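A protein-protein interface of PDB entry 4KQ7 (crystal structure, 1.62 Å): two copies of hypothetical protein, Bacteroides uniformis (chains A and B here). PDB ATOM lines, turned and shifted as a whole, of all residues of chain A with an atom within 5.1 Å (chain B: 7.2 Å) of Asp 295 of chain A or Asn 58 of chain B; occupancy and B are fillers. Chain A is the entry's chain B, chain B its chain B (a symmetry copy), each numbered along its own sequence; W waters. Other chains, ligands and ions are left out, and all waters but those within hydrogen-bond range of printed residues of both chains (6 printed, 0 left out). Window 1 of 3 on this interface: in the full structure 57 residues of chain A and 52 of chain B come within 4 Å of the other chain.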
ATOM      1  N   ARG A 290       0.996  16.964  16.742  1.00  0.00           N
ATOM      2  CA  ARG A 290       2.140  16.391  17.446  1.00  0.00           C
ATOM      3  C   ARG A 290       3.306  17.321  17.264  1.00  0.00           C
ATOM      4  O   ARG A 290       3.633  17.679  16.129  1.00  0.00           O
ATOM      5  CB  ARG A 290       2.495  14.954  17.009  1.00  0.00           C
ATOM      6  CG  ARG A 290       3.676  14.399  17.824  1.00  0.00           C
ATOM      7  CD  ARG A 290       3.903  12.926  17.552  1.00  0.00           C
ATOM      8  NE  ARG A 290       5.188  12.499  18.120  1.00  0.00           N
ATOM      9  CZ  ARG A 290       5.828  11.390  17.779  1.00  0.00           C
ATOM     10  NH1 ARG A 290       5.285  10.541  16.912  1.00  0.00           N
ATOM     11  NH2 ARG A 290       7.032  11.127  18.289  1.00  0.00           N
ATOM     12  N   PHE A 291       3.930  17.712  18.392  1.00  0.00           N
ATOM     13  CA  PHE A 291       5.143  18.526  18.393  1.00  0.00           C
ATOM     14  C   PHE A 291       6.320  17.653  18.793  1.00  0.00           C
ATOM     15  O   PHE A 291       6.215  16.835  19.708  1.00  0.00           O
ATOM     16  CB  PHE A 291       4.974  19.768  19.306  1.00  0.00           C
ATOM     17  CG  PHE A 291       3.924  20.680  18.709  1.00  0.00           C
ATOM     18  CD1 PHE A 291       4.183  21.397  17.538  1.00  0.00           C
ATOM     19  CD2 PHE A 291       2.651  20.753  19.260  1.00  0.00           C
ATOM     20  CE1 PHE A 291       3.181  22.167  16.929  1.00  0.00           C
ATOM     21  CE2 PHE A 291       1.655  21.548  18.673  1.00  0.00           C
ATOM     22  CZ  PHE A 291       1.920  22.232  17.497  1.00  0.00           C
ATOM     23  N   PHE A 292       7.416  17.790  18.056  1.00  0.00           N
ATOM     24  CA  PHE A 292       8.654  17.029  18.209  1.00  0.00           C
ATOM     25  C   PHE A 292       9.688  17.968  18.828  1.00  0.00           C
ATOM     26  O   PHE A 292      10.590  18.465  18.151  1.00  0.00           O
ATOM     27  CB  PHE A 292       9.093  16.462  16.844  1.00  0.00           C
ATOM     28  CG  PHE A 292       8.113  15.498  16.208  1.00  0.00           C
ATOM     29  CD1 PHE A 292       6.960  15.964  15.571  1.00  0.00           C
ATOM     30  CD2 PHE A 292       8.373  14.130  16.183  1.00  0.00           C
ATOM     31  CE1 PHE A 292       6.055  15.074  14.984  1.00  0.00           C
ATOM     32  CE2 PHE A 292       7.473  13.244  15.577  1.00  0.00           C
ATOM     33  CZ  PHE A 292       6.326  13.722  14.982  1.00  0.00           C
ATOM     34  N   ILE A 293       9.498  18.259  20.122  1.00  0.00           N
ATOM     35  CA  ILE A 293      10.342  19.195  20.872  1.00  0.00           C
ATOM     36  C   ILE A 293      11.494  18.439  21.523  1.00  0.00           C
ATOM     37  O   ILE A 293      12.667  18.800  21.348  1.00  0.00           O
ATOM     38  CB  ILE A 293       9.475  19.960  21.914  1.00  0.00           C
ATOM     39  CG1 ILE A 293       8.179  20.601  21.309  1.00  0.00           C
ATOM     40  CG2 ILE A 293      10.308  20.971  22.710  1.00  0.00           C
ATOM     41  CD1 ILE A 293       8.326  21.491  20.181  1.00  0.00           C
ATOM     42  N   GLU A 294      11.151  17.374  22.265  1.00  0.00           N
ATOM     43  CA  GLU A 294      12.158  16.516  22.870  1.00  0.00           C
ATOM     44  C   GLU A 294      12.755  15.586  21.839  1.00  0.00           C
ATOM     45  O   GLU A 294      13.872  15.092  22.032  1.00  0.00           O
ATOM     46  CB  GLU A 294      11.545  15.653  23.995  1.00  0.00           C
ATOM     47  CG  GLU A 294      10.793  16.436  25.053  1.00  0.00           C
ATOM     48  CD  GLU A 294      11.547  17.625  25.617  1.00  0.00           C
ATOM     49  OE1 GLU A 294      12.413  17.418  26.492  1.00  0.00           O
ATOM     50  OE2 GLU A 294      11.329  18.756  25.131  1.00  0.00           O
ATOM     51  N   ASP A 295      11.989  15.306  20.756  1.00  0.00           N
ATOM     52  CA  ASP A 295      12.371  14.281  19.771  1.00  0.00           C
ATOM     53  C   ASP A 295      12.230  14.776  18.318  1.00  0.00           C
ATOM     54  O   ASP A 295      11.483  14.186  17.523  1.00  0.00           O
ATOM     55  CB  ASP A 295      11.477  13.036  20.008  1.00  0.00           C
ATOM     56  CG  ASP A 295       9.968  13.267  19.888  1.00  0.00           C
ATOM     57  OD1 ASP A 295       9.506  14.412  20.165  1.00  0.00           O
ATOM     58  OD2 ASP A 295       9.247  12.303  19.571  1.00  0.00           O
ATOM     59  N   PRO A 296      12.979  15.832  17.929  1.00  0.00           N
ATOM     60  CA  PRO A 296      12.863  16.336  16.540  1.00  0.00           C
ATOM     61  C   PRO A 296      13.352  15.344  15.503  1.00  0.00           C
ATOM     62  O   PRO A 296      14.064  14.390  15.839  1.00  0.00           O
ATOM     63  CB  PRO A 296      13.763  17.591  16.529  1.00  0.00           C
ATOM     64  CG  PRO A 296      13.951  17.954  18.019  1.00  0.00           C
ATOM     65  CD  PRO A 296      13.956  16.617  18.713  1.00  0.00           C
ATOM     66  N   ILE A 297      12.956  15.572  14.235  1.00  0.00           N
ATOM     67  CA  ILE A 297      13.454  14.737  13.145  1.00  0.00           C
ATOM     68  C   ILE A 297      14.538  15.566  12.420  1.00  0.00           C
ATOM     69  O   ILE A 297      14.231  16.514  11.691  1.00  0.00           O
ATOM     70  CB  ILE A 297      12.339  14.197  12.217  1.00  0.00           C
ATOM     71  CG1 ILE A 297      11.405  13.276  13.056  1.00  0.00           C
ATOM     72  CG2 ILE A 297      12.985  13.415  11.049  1.00  0.00           C
ATOM     73  CD1 ILE A 297      10.125  12.934  12.469  1.00  0.00           C
ATOM     74  N   LEU B  12      15.555  24.925  21.275  1.00  0.00           N
ATOM     75  CA  LEU B  12      14.996  24.151  20.152  1.00  0.00           C
ATOM     76  C   LEU B  12      15.388  24.788  18.820  1.00  0.00           C
ATOM     77  O   LEU B  12      15.550  24.078  17.827  1.00  0.00           O
ATOM     78  CB  LEU B  12      13.460  24.082  20.258  1.00  0.00           C
ATOM     79  CG  LEU B  12      12.748  23.225  19.183  1.00  0.00           C
ATOM     80  CD1 LEU B  12      13.119  21.703  19.316  1.00  0.00           C
ATOM     81  CD2 LEU B  12      11.236  23.394  19.287  1.00  0.00           C
ATOM     82  N   ASN B  21      18.503  10.464  13.271  1.00  0.00           N
ATOM     83  CA  ASN B  21      17.308   9.707  13.649  1.00  0.00           C
ATOM     84  C   ASN B  21      17.324   8.306  13.122  1.00  0.00           C
ATOM     85  O   ASN B  21      17.687   8.060  11.969  1.00  0.00           O
ATOM     86  CB  ASN B  21      16.024  10.357  13.160  1.00  0.00           C
ATOM     87  CG  ASN B  21      15.666  11.598  13.922  1.00  0.00           C
ATOM     88  OD1 ASN B  21      14.705  11.639  14.725  1.00  0.00           O
ATOM     89  ND2 ASN B  21      16.393  12.625  13.619  1.00  0.00           N
ATOM     90  N   LYS B  22      16.860   7.390  13.985  1.00  0.00           N
ATOM     91  CA  LYS B  22      16.607   5.995  13.646  1.00  0.00           C
ATOM     92  C   LYS B  22      15.284   5.616  14.272  1.00  0.00           C
ATOM     93  O   LYS B  22      14.850   6.244  15.248  1.00  0.00           O
ATOM     94  CB  LYS B  22      17.737   5.076  14.133  1.00  0.00           C
ATOM     95  CG  LYS B  22      19.123   5.383  13.565  1.00  0.00           C
ATOM     96  CD  LYS B  22      19.250   4.911  12.138  1.00  0.00           C
ATOM     97  CE  LYS B  22      20.611   5.219  11.576  1.00  0.00           C
ATOM     98  NZ  LYS B  22      20.889   4.408  10.365  1.00  0.00           N
ATOM     99  N   VAL B  56      20.613   7.340  21.924  1.00  0.00           N
ATOM    100  CA  VAL B  56      19.701   7.746  22.992  1.00  0.00           C
ATOM    101  C   VAL B  56      18.286   7.522  22.505  1.00  0.00           C
ATOM    102  O   VAL B  56      17.864   8.172  21.538  1.00  0.00           O
ATOM    103  CB  VAL B  56      19.905   9.233  23.441  1.00  0.00           C
ATOM    104  CG1 VAL B  56      18.908   9.605  24.531  1.00  0.00           C
ATOM    105  CG2 VAL B  56      21.337   9.503  23.924  1.00  0.00           C
ATOM    106  N   ILE B  57      17.546   6.613  23.156  1.00  0.00           N
ATOM    107  CA  ILE B  57      16.118   6.451  22.838  1.00  0.00           C
ATOM    108  C   ILE B  57      15.409   7.673  23.404  1.00  0.00           C
ATOM    109  O   ILE B  57      15.672   8.032  24.556  1.00  0.00           O
ATOM    110  CB  ILE B  57      15.558   5.130  23.431  1.00  0.00           C
ATOM    111  CG1 ILE B  57      16.157   3.906  22.717  1.00  0.00           C
ATOM    112  CG2 ILE B  57      14.016   5.083  23.370  1.00  0.00           C
ATOM    113  CD1 ILE B  57      16.020   2.594  23.574  1.00  0.00           C
ATOM    114  N   ASN B  58      14.507   8.316  22.619  1.00  0.00           N
ATOM    115  CA  ASN B  58      13.856   9.498  23.181  1.00  0.00           C
ATOM    116  C   ASN B  58      12.358   9.529  22.918  1.00  0.00           C
ATOM    117  O   ASN B  58      11.710  10.510  23.280  1.00  0.00           O
ATOM    118  CB  ASN B  58      14.532  10.788  22.702  1.00  0.00           C
ATOM    119  CG  ASN B  58      14.611  10.931  21.200  1.00  0.00           C
ATOM    120  OD1 ASN B  58      14.090  10.107  20.433  1.00  0.00           O
ATOM    121  ND2 ASN B  58      15.218  12.012  20.749  1.00  0.00           N
ATOM    122  N   HIS B  59      11.788   8.452  22.336  1.00  0.00           N
ATOM    123  CA  HIS B  59      10.336   8.338  22.183  1.00  0.00           C
ATOM    124  C   HIS B  59       9.979   6.890  21.952  1.00  0.00           C
ATOM    125  O   HIS B  59      10.513   6.258  21.030  1.00  0.00           O
ATOM    126  CB  HIS B  59       9.781   9.227  21.039  1.00  0.00           C
ATOM    127  CG  HIS B  59       8.361   8.903  20.658  1.00  0.00           C
ATOM    128  ND1 HIS B  59       8.075   8.113  19.548  1.00  0.00           N
ATOM    129  CD2 HIS B  59       7.198   9.254  21.252  1.00  0.00           C
ATOM    130  CE1 HIS B  59       6.753   8.039  19.493  1.00  0.00           C
ATOM    131  NE2 HIS B  59       6.186   8.693  20.504  1.00  0.00           N
ATOM    132  N   ILE B  60       9.067   6.370  22.785  1.00  0.00           N
ATOM    133  CA  ILE B  60       8.522   5.030  22.620  1.00  0.00           C
ATOM    134  C   ILE B  60       7.013   5.143  22.597  1.00  0.00           C
ATOM    135  O   ILE B  60       6.456   5.836  23.436  1.00  0.00           O
ATOM    136  CB  ILE B  60       8.972   4.060  23.752  1.00  0.00           C
ATOM    137  CG1 ILE B  60      10.514   3.928  23.811  1.00  0.00           C
ATOM    138  CG2 ILE B  60       8.279   2.673  23.623  1.00  0.00           C
ATOM    139  CD1 ILE B  60      11.014   3.088  25.024  1.00  0.00           C
ATOM    140  N   CYS B 125       6.084   7.270  25.886  1.00  0.00           N
ATOM    141  CA  CYS B 125       7.139   7.538  26.864  1.00  0.00           C
ATOM    142  C   CYS B 125       8.181   8.480  26.250  1.00  0.00           C
ATOM    143  O   CYS B 125       8.686   8.195  25.165  1.00  0.00           O
ATOM    144  CB  CYS B 125       7.768   6.215  27.313  1.00  0.00           C
ATOM    145  SG  CYS B 125       9.263   6.391  28.340  1.00  0.00           S
ATOM    146  N   TYR B 126       8.521   9.577  26.967  1.00  0.00           N
ATOM    147  CA  TYR B 126       9.517  10.545  26.520  1.00  0.00           C
ATOM    148  C   TYR B 126      10.768  10.557  27.415  1.00  0.00           C
ATOM    149  O   TYR B 126      11.573  11.480  27.298  1.00  0.00           O
ATOM    150  CB  TYR B 126       8.913  11.965  26.429  1.00  0.00           C
ATOM    151  CG  TYR B 126       8.037  12.138  25.209  1.00  0.00           C
ATOM    152  CD1 TYR B 126       8.590  12.451  23.967  1.00  0.00           C
ATOM    153  CD2 TYR B 126       6.651  12.014  25.297  1.00  0.00           C
ATOM    154  CE1 TYR B 126       7.783  12.609  22.835  1.00  0.00           C
ATOM    155  CE2 TYR B 126       5.840  12.160  24.174  1.00  0.00           C
ATOM    156  CZ  TYR B 126       6.408  12.475  22.951  1.00  0.00           C
ATOM    157  OH  TYR B 126       5.611  12.670  21.848  1.00  0.00           O
ATOM    158  N   PHE B 127      10.949   9.554  28.303  1.00  0.00           N
ATOM    159  CA  PHE B 127      12.217   9.491  29.032  1.00  0.00           C
ATOM    160  C   PHE B 127      13.352   9.214  28.041  1.00  0.00           C
ATOM    161  O   PHE B 127      13.196   8.373  27.144  1.00  0.00           O
ATOM    162  CB  PHE B 127      12.201   8.377  30.093  1.00  0.00           C
ATOM    163  CG  PHE B 127      11.493   8.730  31.376  1.00  0.00           C
ATOM    164  CD1 PHE B 127      11.951   9.779  32.181  1.00  0.00           C
ATOM    165  CD2 PHE B 127      10.416   7.974  31.822  1.00  0.00           C
ATOM    166  CE1 PHE B 127      11.320  10.081  33.395  1.00  0.00           C
ATOM    167  CE2 PHE B 127       9.785   8.276  33.034  1.00  0.00           C
ATOM    168  CZ  PHE B 127      10.242   9.324  33.815  1.00  0.00           C
ATOM    169  N   ALA B 128      14.479   9.911  28.201  1.00  0.00           N
ATOM    170  CA  ALA B 128      15.655   9.699  27.347  1.00  0.00           C
ATOM    171  C   ALA B 128      16.462   8.527  27.922  1.00  0.00           C
ATOM    172  O   ALA B 128      16.653   8.443  29.144  1.00  0.00           O
ATOM    173  CB  ALA B 128      16.496  10.965  27.273  1.00  0.00           C
ATOM    174  N   MET B 129      16.894   7.597  27.049  1.00  0.00           N
ATOM    175  CA  MET B 129      17.572   6.382  27.504  1.00  0.00           C
ATOM    176  C   MET B 129      18.866   6.194  26.735  1.00  0.00           C
ATOM    177  O   MET B 129      18.864   5.630  25.625  1.00  0.00           O
ATOM    178  CB  MET B 129      16.656   5.155  27.357  1.00  0.00           C
ATOM    179  CG  MET B 129      15.249   5.411  27.891  1.00  0.00           C
ATOM    180  SD  MET B 129      14.133   3.848  27.644  1.00  0.00           S
ATOM    181  CE  MET B 129      12.440   4.601  28.191  1.00  0.00           C
ATOM    182  N   VAL B 154      10.016   2.646  18.383  1.00  0.00           N
ATOM    183  CA  VAL B 154      11.160   2.948  19.250  1.00  0.00           C
ATOM    184  C   VAL B 154      11.983   3.943  18.448  1.00  0.00           C
ATOM    185  O   VAL B 154      12.617   3.555  17.465  1.00  0.00           O
ATOM    186  CB  VAL B 154      11.982   1.726  19.731  1.00  0.00           C
ATOM    187  CG1 VAL B 154      13.280   2.186  20.420  1.00  0.00           C
ATOM    188  CG2 VAL B 154      11.154   0.866  20.688  1.00  0.00           C
ATOM    189  N   ASP B 155      11.867   5.235  18.804  1.00  0.00           N
ATOM    190  CA  ASP B 155      12.583   6.330  18.139  1.00  0.00           C
ATOM    191  C   ASP B 155      13.826   6.653  18.912  1.00  0.00           C
ATOM    192  O   ASP B 155      13.770   6.825  20.135  1.00  0.00           O
ATOM    193  CB  ASP B 155      11.689   7.581  18.048  1.00  0.00           C
ATOM    194  CG  ASP B 155      10.611   7.423  17.001  1.00  0.00           C
ATOM    195  OD1 ASP B 155      10.931   7.564  15.792  1.00  0.00           O
ATOM    196  OD2 ASP B 155       9.437   7.188  17.385  1.00  0.00           O
ATOM    197  N   TYR B 156      14.954   6.754  18.217  1.00  0.00           N
ATOM    198  CA  TYR B 156      16.189   7.063  18.924  1.00  0.00           C
ATOM    199  C   TYR B 156      17.130   7.852  18.049  1.00  0.00           C
ATOM    200  O   TYR B 156      16.928   7.966  16.829  1.00  0.00           O
ATOM    201  CB  TYR B 156      16.868   5.774  19.453  1.00  0.00           C
ATOM    202  CG  TYR B 156      17.440   4.858  18.392  1.00  0.00           C
ATOM    203  CD1 TYR B 156      16.635   3.921  17.742  1.00  0.00           C
ATOM    204  CD2 TYR B 156      18.803   4.864  18.101  1.00  0.00           C
ATOM    205  CE1 TYR B 156      17.174   3.027  16.808  1.00  0.00           C
ATOM    206  CE2 TYR B 156      19.348   3.976  17.180  1.00  0.00           C
ATOM    207  CZ  TYR B 156      18.534   3.054  16.543  1.00  0.00           C
ATOM    208  OH  TYR B 156      19.094   2.202  15.622  1.00  0.00           O
ATOM    209  N   LEU B 157      18.142   8.445  18.690  1.00  0.00           N
ATOM    210  CA  LEU B 157      19.195   9.175  17.995  1.00  0.00           C
ATOM    211  C   LEU B 157      20.468   8.369  18.034  1.00  0.00           C
ATOM    212  O   LEU B 157      20.959   8.034  19.119  1.00  0.00           O
ATOM    213  CB  LEU B 157      19.426  10.583  18.594  1.00  0.00           C
ATOM    214  CG  LEU B 157      18.223  11.534  18.495  1.00  0.00           C
ATOM    215  CD1 LEU B 157      18.438  12.783  19.340  1.00  0.00           C
ATOM    216  CD2 LEU B 157      17.923  11.909  17.017  1.00  0.00           C
HETATM  217  O   HOH W   1      14.925  13.011  18.055  1.00  0.00           O
HETATM  218  O   HOH W   2      11.819  11.584  16.377  1.00  0.00           O
HETATM  219  O   HOH W   3       7.812   9.032  16.059  1.00  0.00           O
HETATM  220  O   HOH W   4       6.806  14.158  19.944  1.00  0.00           O
HETATM  221  O   HOH W   5      16.283  13.760  22.595  1.00  0.00           O
HETATM  222  O   HOH W   6      10.038  10.382  17.873  1.00  0.00           O
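Of chain B, only Asn 58 (3.8 Å), His 59 (3.4 Å) and Tyr 126 (3.6 Å) come within 4 Å of Asp 295 of chain A. Of chain A, only Glu 294 and Asp 295 come within 4 Å of Asn 58 of chain B. Of the printed residues of chain B, Glu 294 of chain A touches Asn 58 (3.6 Å). Printed residues of chain B within 4 Å of Pro 296 of chain A: Asn 21 (3.0 Å). Tyr 156 of chain B touches none of the printed residues of chain A. Ile 57 of chain B touches none of the printed residues of chain A. The nearest printed residue of chain A that does not touch Asn 58 of chain B is Pro 296 of chain A (5.2 Å). The nearest printed residue of chain B that does not touch Ile 297 of chain A is Asp 155 of chain B (6.4 Å).
NH2 of Arg 290 of chain A lies within salt-bridge range of OD2 of Asp 295 of chain A (2.8 Å). The backbone NH (N) of Asn 58 of chain B is in hydrogen-bond range of the backbone carbonyl oxygen (O) of Asp 155 of chain B (3.0 Å). ND1 of His 59 of chain B lies within hydrogen-bond range of OD2 of Asp 155 of chain B (2.7 Å).
Among the printed residues, merely in contact across the chains: Asp 295 of chain A with His 59 of chain B (3.4 Å), Ile 293 of chain A with Leu 12 of chain B (3.6 Å), Asp 295 of chain A with Tyr 126 of chain B (3.6 Å), Glu 294 of chain A with Asn 58 of chain B (3.6 Å), Ile 297 of chain A with Asn 21 of chain B (3.7 Å), Arg 290 of chain A with Tyr 126 of chain B (3.8 Å) and Asp 295 of chain A with Asn 58 of chain B (3.8 Å).
No position is printed for both chains. Of the 9 pairs that touch across the chains among the printed residues, none has its exchanged pair printed and touching as well.
Printed residues of chain A that touch a printed residue of chain B: Arg 290, Ile 293, Glu 294, Asp 295, Pro 296 and Ile 297. Of the 17 printed residues of chain B, 5 touch a printed residue of chain A. Hydrophobic or aromatic side chains of chain B within 4 Å of the printed part of chain A: Leu 12, His 59 and Tyr 126. Along chain B the printed residues that touch a printed residue of chain A span positions 12 to 126.
Water W6 lies within hydrogen-bond range of the side-chain carboxylate of Asp 295 of chain A (2.7 Å), the guanidinium group of Arg 290 of chain A (3.1 Å), the side-chain carboxylate of Asp 155 of chain B (3.3 Å) and a ring nitrogen (ND1) of His 59 of chain B (3.4 Å). Water W4 lies within hydrogen-bond range of OH of Tyr 126 of chain B (2.7 Å), OD1 of Asp 295 of chain A (2.7 Å), O of Phe 291 of chain A (2.8 Å) and NE of Arg 290 of chain A (2.9 Å). Water W1 lies within hydrogen-bond range of O of Pro 296 of chain A and ND2 of Asn 58 of chain B. Water W5 lies within hydrogen-bond range of the side-chain amide nitrogen (ND2) of Asn 58 of chain B (2.8 Å) and the backbone carbonyl oxygen (O) of Glu 294 of chain A (2.8 Å). Water W3 lies within hydrogen-bond range of the side-chain carboxylate of Asp 155 of chain B and the guanidinium group of Arg 290 of chain A. Water W2 bridges O of Asp 295 of chain A (2.9 Å) and OD1 of Asn 21 of chain B (3.3 Å).
The guanidinium group (NH2) of Arg 290 of chain A sits close to a ring nitrogen (NE2) of His 59 of chain B. The backbone carbonyl oxygen (O) of Pro 296 of chain A lies close to the side-chain amide oxygen (OD1) of Asn 21 of chain B (3.0 Å).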
